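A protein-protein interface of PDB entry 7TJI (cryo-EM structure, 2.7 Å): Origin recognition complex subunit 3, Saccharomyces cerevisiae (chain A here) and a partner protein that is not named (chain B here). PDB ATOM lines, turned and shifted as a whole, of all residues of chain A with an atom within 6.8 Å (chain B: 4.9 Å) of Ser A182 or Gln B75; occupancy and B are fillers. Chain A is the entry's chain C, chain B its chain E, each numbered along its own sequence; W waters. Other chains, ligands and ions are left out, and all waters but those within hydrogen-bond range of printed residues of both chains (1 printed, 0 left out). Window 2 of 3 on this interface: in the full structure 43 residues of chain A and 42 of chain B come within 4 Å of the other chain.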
ATOM      1  N   ARG A 144      18.248  13.541  23.699  1.00  0.00           N
ATOM      2  CA  ARG A 144      17.500  13.258  24.922  1.00  0.00           C
ATOM      3  C   ARG A 144      16.824  14.506  25.480  1.00  0.00           C
ATOM      4  O   ARG A 144      15.657  14.447  25.885  1.00  0.00           O
ATOM      5  CB  ARG A 144      18.417  12.627  25.966  1.00  0.00           C
ATOM      6  CG  ARG A 144      18.723  11.170  25.692  1.00  0.00           C
ATOM      7  CD  ARG A 144      19.689  10.587  26.707  1.00  0.00           C
ATOM      8  NE  ARG A 144      19.085  10.455  28.025  1.00  0.00           N
ATOM      9  CZ  ARG A 144      18.250   9.490  28.384  1.00  0.00           C
ATOM     10  NH1 ARG A 144      17.896   8.531  27.546  1.00  0.00           N
ATOM     11  NH2 ARG A 144      17.759   9.485  29.619  1.00  0.00           N
ATOM     12  N   MET A 147      13.858  15.326  23.057  1.00  0.00           N
ATOM     13  CA  MET A 147      12.691  14.466  23.217  1.00  0.00           C
ATOM     14  C   MET A 147      12.019  14.633  24.570  1.00  0.00           C
ATOM     15  O   MET A 147      10.792  14.512  24.650  1.00  0.00           O
ATOM     16  CB  MET A 147      13.064  13.001  22.974  1.00  0.00           C
ATOM     17  CG  MET A 147      13.632  12.612  21.586  1.00  0.00           C
ATOM     18  SD  MET A 147      12.681  12.889  20.052  1.00  0.00           S
ATOM     19  CE  MET A 147      12.862  14.629  19.634  1.00  0.00           C
ATOM     20  N   ASP A 180       5.072   6.582  30.457  1.00  0.00           N
ATOM     21  CA  ASP A 180       6.417   7.004  30.101  1.00  0.00           C
ATOM     22  C   ASP A 180       6.845   6.385  28.778  1.00  0.00           C
ATOM     23  O   ASP A 180       6.475   5.257  28.446  1.00  0.00           O
ATOM     24  CB  ASP A 180       7.410   6.627  31.201  1.00  0.00           C
ATOM     25  CG  ASP A 180       6.955   7.075  32.576  1.00  0.00           C
ATOM     26  OD1 ASP A 180       6.857   8.299  32.808  1.00  0.00           O
ATOM     27  OD2 ASP A 180       6.693   6.202  33.429  1.00  0.00           O
ATOM     28  N   VAL A 181       7.623   7.147  28.014  1.00  0.00           N
ATOM     29  CA  VAL A 181       8.217   6.677  26.773  1.00  0.00           C
ATOM     30  C   VAL A 181       9.730   6.806  26.891  1.00  0.00           C
ATOM     31  O   VAL A 181      10.256   7.400  27.830  1.00  0.00           O
ATOM     32  CB  VAL A 181       7.700   7.444  25.538  1.00  0.00           C
ATOM     33  CG1 VAL A 181       6.203   7.261  25.377  1.00  0.00           C
ATOM     34  CG2 VAL A 181       8.059   8.916  25.635  1.00  0.00           C
ATOM     35  N   SER A 182      10.428   6.234  25.917  1.00  0.00           N
ATOM     36  CA  SER A 182      11.874   6.366  25.825  1.00  0.00           C
ATOM     37  C   SER A 182      12.215   7.597  24.994  1.00  0.00           C
ATOM     38  O   SER A 182      11.678   7.782  23.898  1.00  0.00           O
ATOM     39  CB  SER A 182      12.492   5.111  25.209  1.00  0.00           C
ATOM     40  OG  SER A 182      13.885   5.065  25.443  1.00  0.00           O
ATOM     41  N   TYR A 183      13.113   8.435  25.516  1.00  0.00           N
ATOM     42  CA  TYR A 183      13.433   9.720  24.894  1.00  0.00           C
ATOM     43  C   TYR A 183      14.420   9.503  23.750  1.00  0.00           C
ATOM     44  O   TYR A 183      15.616   9.780  23.845  1.00  0.00           O
ATOM     45  CB  TYR A 183      13.978  10.698  25.926  1.00  0.00           C
ATOM     46  CG  TYR A 183      12.990  11.030  27.012  1.00  0.00           C
ATOM     47  CD1 TYR A 183      11.703  11.443  26.701  1.00  0.00           C
ATOM     48  CD2 TYR A 183      13.341  10.920  28.349  1.00  0.00           C
ATOM     49  CE1 TYR A 183      10.794  11.744  27.694  1.00  0.00           C
ATOM     50  CE2 TYR A 183      12.440  11.215  29.348  1.00  0.00           C
ATOM     51  CZ  TYR A 183      11.172  11.626  29.016  1.00  0.00           C
ATOM     52  OH  TYR A 183      10.281  11.920  30.015  1.00  0.00           O
ATOM     53  N   ASP A 184      13.889   8.999  22.640  1.00  0.00           N
ATOM     54  CA  ASP A 184      14.623   8.881  21.395  1.00  0.00           C
ATOM     55  C   ASP A 184      13.666   9.214  20.258  1.00  0.00           C
ATOM     56  O   ASP A 184      12.509   9.575  20.481  1.00  0.00           O
ATOM     57  CB  ASP A 184      15.257   7.490  21.245  1.00  0.00           C
ATOM     58  CG  ASP A 184      14.278   6.365  21.514  1.00  0.00           C
ATOM     59  OD1 ASP A 184      13.385   6.128  20.682  1.00  0.00           O
ATOM     60  OD2 ASP A 184      14.397   5.719  22.569  1.00  0.00           O
ATOM     61  N   LEU A 185      14.145   9.058  19.029  1.00  0.00           N
ATOM     62  CA  LEU A 185      13.412   9.502  17.852  1.00  0.00           C
ATOM     63  C   LEU A 185      12.257   8.582  17.467  1.00  0.00           C
ATOM     64  O   LEU A 185      11.552   8.880  16.498  1.00  0.00           O
ATOM     65  CB  LEU A 185      14.374   9.659  16.673  1.00  0.00           C
ATOM     66  CG  LEU A 185      14.169  10.873  15.764  1.00  0.00           C
ATOM     67  CD1 LEU A 185      14.007  12.153  16.575  1.00  0.00           C
ATOM     68  CD2 LEU A 185      15.329  10.999  14.799  1.00  0.00           C
ATOM     69  N   SER A 186      12.039   7.479  18.188  1.00  0.00           N
ATOM     70  CA  SER A 186      10.818   6.708  18.003  1.00  0.00           C
ATOM     71  C   SER A 186       9.611   7.397  18.621  1.00  0.00           C
ATOM     72  O   SER A 186       8.475   7.049  18.283  1.00  0.00           O
ATOM     73  CB  SER A 186      10.976   5.303  18.588  1.00  0.00           C
ATOM     74  OG  SER A 186      11.351   5.350  19.953  1.00  0.00           O
ATOM     75  N   LEU A 187       9.834   8.351  19.527  1.00  0.00           N
ATOM     76  CA  LEU A 187       8.752   9.204  20.006  1.00  0.00           C
ATOM     77  C   LEU A 187       8.236  10.107  18.890  1.00  0.00           C
ATOM     78  O   LEU A 187       7.035  10.388  18.812  1.00  0.00           O
ATOM     79  CB  LEU A 187       9.239  10.025  21.198  1.00  0.00           C
ATOM     80  CG  LEU A 187       8.385  11.183  21.702  1.00  0.00           C
ATOM     81  CD1 LEU A 187       7.119  10.655  22.351  1.00  0.00           C
ATOM     82  CD2 LEU A 187       9.174  12.046  22.669  1.00  0.00           C
ATOM     83  N   LYS B  71      20.538   0.869  25.544  1.00  0.00           N
ATOM     84  CA  LYS B  71      19.312   0.699  26.323  1.00  0.00           C
ATOM     85  C   LYS B  71      18.036   1.036  25.545  1.00  0.00           C
ATOM     86  O   LYS B  71      17.089   0.227  25.602  1.00  0.00           O
ATOM     87  CB  LYS B  71      19.455   1.487  27.637  1.00  0.00           C
ATOM     88  CG  LYS B  71      18.336   1.330  28.645  1.00  0.00           C
ATOM     89  CD  LYS B  71      18.784   1.908  29.976  1.00  0.00           C
ATOM     90  CE  LYS B  71      17.626   2.189  30.898  1.00  0.00           C
ATOM     91  NZ  LYS B  71      18.077   2.250  32.317  1.00  0.00           N
ATOM     92  N   PRO B  72      17.924   2.164  24.804  1.00  0.00           N
ATOM     93  CA  PRO B  72      16.748   2.318  23.930  1.00  0.00           C
ATOM     94  C   PRO B  72      16.651   1.279  22.830  1.00  0.00           C
ATOM     95  O   PRO B  72      15.539   0.979  22.395  1.00  0.00           O
ATOM     96  CB  PRO B  72      16.923   3.727  23.347  1.00  0.00           C
ATOM     97  CG  PRO B  72      17.728   4.423  24.312  1.00  0.00           C
ATOM     98  CD  PRO B  72      18.705   3.422  24.786  1.00  0.00           C
ATOM     99  N   LEU B  73      17.772   0.713  22.378  1.00  0.00           N
ATOM    100  CA  LEU B  73      17.722  -0.353  21.382  1.00  0.00           C
ATOM    101  C   LEU B  73      17.105  -1.627  21.957  1.00  0.00           C
ATOM    102  O   LEU B  73      16.279  -2.273  21.297  1.00  0.00           O
ATOM    103  CB  LEU B  73      19.125  -0.612  20.837  1.00  0.00           C
ATOM    104  CG  LEU B  73      19.359  -1.776  19.873  1.00  0.00           C
ATOM    105  CD1 LEU B  73      18.470  -1.678  18.650  1.00  0.00           C
ATOM    106  CD2 LEU B  73      20.816  -1.819  19.475  1.00  0.00           C
ATOM    107  N   LEU B  74      17.480  -1.988  23.192  1.00  0.00           N
ATOM    108  CA  LEU B  74      16.867  -3.134  23.864  1.00  0.00           C
ATOM    109  C   LEU B  74      15.376  -2.917  24.096  1.00  0.00           C
ATOM    110  O   LEU B  74      14.558  -3.822  23.852  1.00  0.00           O
ATOM    111  CB  LEU B  74      17.559  -3.403  25.198  1.00  0.00           C
ATOM    112  CG  LEU B  74      19.048  -3.726  25.287  1.00  0.00           C
ATOM    113  CD1 LEU B  74      19.473  -3.766  26.741  1.00  0.00           C
ATOM    114  CD2 LEU B  74      19.378  -5.033  24.596  1.00  0.00           C
ATOM    115  N   GLN B  75      15.002  -1.712  24.548  1.00  0.00           N
ATOM    116  CA  GLN B  75      13.591  -1.411  24.775  1.00  0.00           C
ATOM    117  C   GLN B  75      12.804  -1.374  23.468  1.00  0.00           C
ATOM    118  O   GLN B  75      11.642  -1.797  23.429  1.00  0.00           O
ATOM    119  CB  GLN B  75      13.453  -0.096  25.537  1.00  0.00           C
ATOM    120  CG  GLN B  75      14.105  -0.134  26.898  1.00  0.00           C
ATOM    121  CD  GLN B  75      14.269   1.229  27.517  1.00  0.00           C
ATOM    122  OE1 GLN B  75      14.233   2.244  26.830  1.00  0.00           O
ATOM    123  NE2 GLN B  75      14.468   1.259  28.826  1.00  0.00           N
ATOM    124  N   ALA B  76      13.430  -0.906  22.386  1.00  0.00           N
ATOM    125  CA  ALA B  76      12.783  -0.898  21.079  1.00  0.00           C
ATOM    126  C   ALA B  76      12.546  -2.310  20.564  1.00  0.00           C
ATOM    127  O   ALA B  76      11.500  -2.583  19.961  1.00  0.00           O
ATOM    128  CB  ALA B  76      13.625  -0.101  20.088  1.00  0.00           C
ATOM    129  N   ILE B  77      13.505  -3.214  20.796  1.00  0.00           N
ATOM    130  CA  ILE B  77      13.332  -4.613  20.405  1.00  0.00           C
ATOM    131  C   ILE B  77      12.170  -5.236  21.170  1.00  0.00           C
ATOM    132  O   ILE B  77      11.272  -5.852  20.573  1.00  0.00           O
ATOM    133  CB  ILE B  77      14.645  -5.394  20.618  1.00  0.00           C
ATOM    134  CG1 ILE B  77      15.626  -5.108  19.484  1.00  0.00           C
ATOM    135  CG2 ILE B  77      14.402  -6.899  20.727  1.00  0.00           C
ATOM    136  CD1 ILE B  77      17.039  -5.499  19.797  1.00  0.00           C
ATOM    137  N   ALA B  78      12.138  -5.030  22.493  1.00  0.00           N
ATOM    138  CA  ALA B  78      11.084  -5.617  23.320  1.00  0.00           C
ATOM    139  C   ALA B  78       9.709  -5.025  23.017  1.00  0.00           C
ATOM    140  O   ALA B  78       8.697  -5.721  23.144  1.00  0.00           O
ATOM    141  CB  ALA B  78      11.411  -5.445  24.802  1.00  0.00           C
ATOM    142  N   ARG B  79       9.655  -3.760  22.603  1.00  0.00           N
ATOM    143  CA  ARG B  79       8.386  -3.152  22.222  1.00  0.00           C
ATOM    144  C   ARG B  79       7.893  -3.682  20.880  1.00  0.00           C
ATOM    145  O   ARG B  79       6.752  -4.160  20.765  1.00  0.00           O
ATOM    146  CB  ARG B  79       8.551  -1.634  22.180  1.00  0.00           C
ATOM    147  CG  ARG B  79       7.336  -0.846  21.748  1.00  0.00           C
ATOM    148  CD  ARG B  79       7.562   0.637  22.001  1.00  0.00           C
ATOM    149  NE  ARG B  79       8.533   1.210  21.077  1.00  0.00           N
ATOM    150  CZ  ARG B  79       9.775   1.548  21.401  1.00  0.00           C
ATOM    151  NH1 ARG B  79      10.233   1.396  22.633  1.00  0.00           N
ATOM    152  NH2 ARG B  79      10.579   2.039  20.464  1.00  0.00           N
ATOM    153  N   PRO B  99       7.998  -2.424  27.869  1.00  0.00           N
ATOM    154  CA  PRO B  99       9.368  -2.453  27.329  1.00  0.00           C
ATOM    155  C   PRO B  99      10.362  -1.622  28.122  1.00  0.00           C
ATOM    156  O   PRO B  99      11.567  -1.870  28.008  1.00  0.00           O
ATOM    157  CB  PRO B  99       9.200  -1.913  25.903  1.00  0.00           C
ATOM    158  CG  PRO B  99       7.909  -1.185  25.912  1.00  0.00           C
ATOM    159  CD  PRO B  99       7.036  -1.881  26.899  1.00  0.00           C
ATOM    160  N   LEU B 100       9.905  -0.670  28.934  1.00  0.00           N
ATOM    161  CA  LEU B 100      10.800   0.096  29.791  1.00  0.00           C
ATOM    162  C   LEU B 100      11.278  -0.690  31.002  1.00  0.00           C
ATOM    163  O   LEU B 100      12.153  -0.204  31.724  1.00  0.00           O
ATOM    164  CB  LEU B 100      10.131   1.393  30.259  1.00  0.00           C
ATOM    165  CG  LEU B 100      10.100   2.674  29.412  1.00  0.00           C
ATOM    166  CD1 LEU B 100       9.978   2.469  27.907  1.00  0.00           C
ATOM    167  CD2 LEU B 100       8.967   3.545  29.907  1.00  0.00           C
ATOM    168  N   VAL B 102      12.928  -3.374  30.543  1.00  0.00           N
ATOM    169  CA  VAL B 102      14.208  -3.867  30.046  1.00  0.00           C
ATOM    170  C   VAL B 102      15.254  -2.776  30.242  1.00  0.00           C
ATOM    171  O   VAL B 102      15.226  -1.751  29.560  1.00  0.00           O
ATOM    172  CB  VAL B 102      14.109  -4.279  28.571  1.00  0.00           C
ATOM    173  CG1 VAL B 102      15.464  -4.731  28.045  1.00  0.00           C
ATOM    174  CG2 VAL B 102      13.070  -5.371  28.394  1.00  0.00           C
HETATM  175  O   HOH W   1      13.183   2.574  22.561  1.00  0.00           O
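The side-chain amide oxygen (OE1) of Gln B75 sits at hydrogen-bond distance from the side-chain hydroxyl (OG) of Ser A182, at 3.2 Å. The side-chain hydroxyl (OG) of Ser A186 lies within hydrogen-bond range of the guanidinium group (NH2) of Arg B79.
Of chain A, only Ser A182 comes within 4 Å of Gln B75. Of the printed residues of chain B, Asp A184 touches Pro B72. Printed residues of chain A within 4 Å of Pro B72: Ser A182 (3.9 Å) and Asp A184 (3.3 Å). Of the printed residues of chain B, Ser A186 touches Arg B79 (3.4 Å). Printed residues of chain A within 4 Å of Arg B79: Ser A186 (3.4 Å). The nearest residue of chain A that does not touch Gln B75 is Asp A184 (5.5 Å).
Asp A180 touches Leu B100. Pro B72 touches Ser A182 (CB to OG, 3.9 Å). Asp A184 touches Pro B72.
The side-chain amide nitrogen (NE2) of Gln B75 lies within hydrogen-bond range of the backbone carbonyl oxygen (O) of Val B102, 3.2 Å away. The side-chain carboxylate of Asp A184 lies within hydrogen-bond range of the backbone NH of Ser A186. The side-chain hydroxyl (OG) of Ser A182 sits at hydrogen-bond distance from the side-chain carboxylate (OD2) of Asp A184 (3.0 Å).
Of the 12 printed residues of chain B, 4 touch a printed residue of chain A. Printed residues of chain B that touch a printed residue of chain A: Pro B72, Gln B75, Arg B79 and Leu B100. Hydrophobic or aromatic side chains of chain B within 4 Å of the printed part of chain A: Pro B72 and Leu B100.
Water W1 lies within hydrogen-bond range of O of Pro B72 (2.8 Å), NH1 of Arg B79 (3.2 Å), OD2 of Asp A184 (3.4 Å) and N of Ala B76 (3.5 Å).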
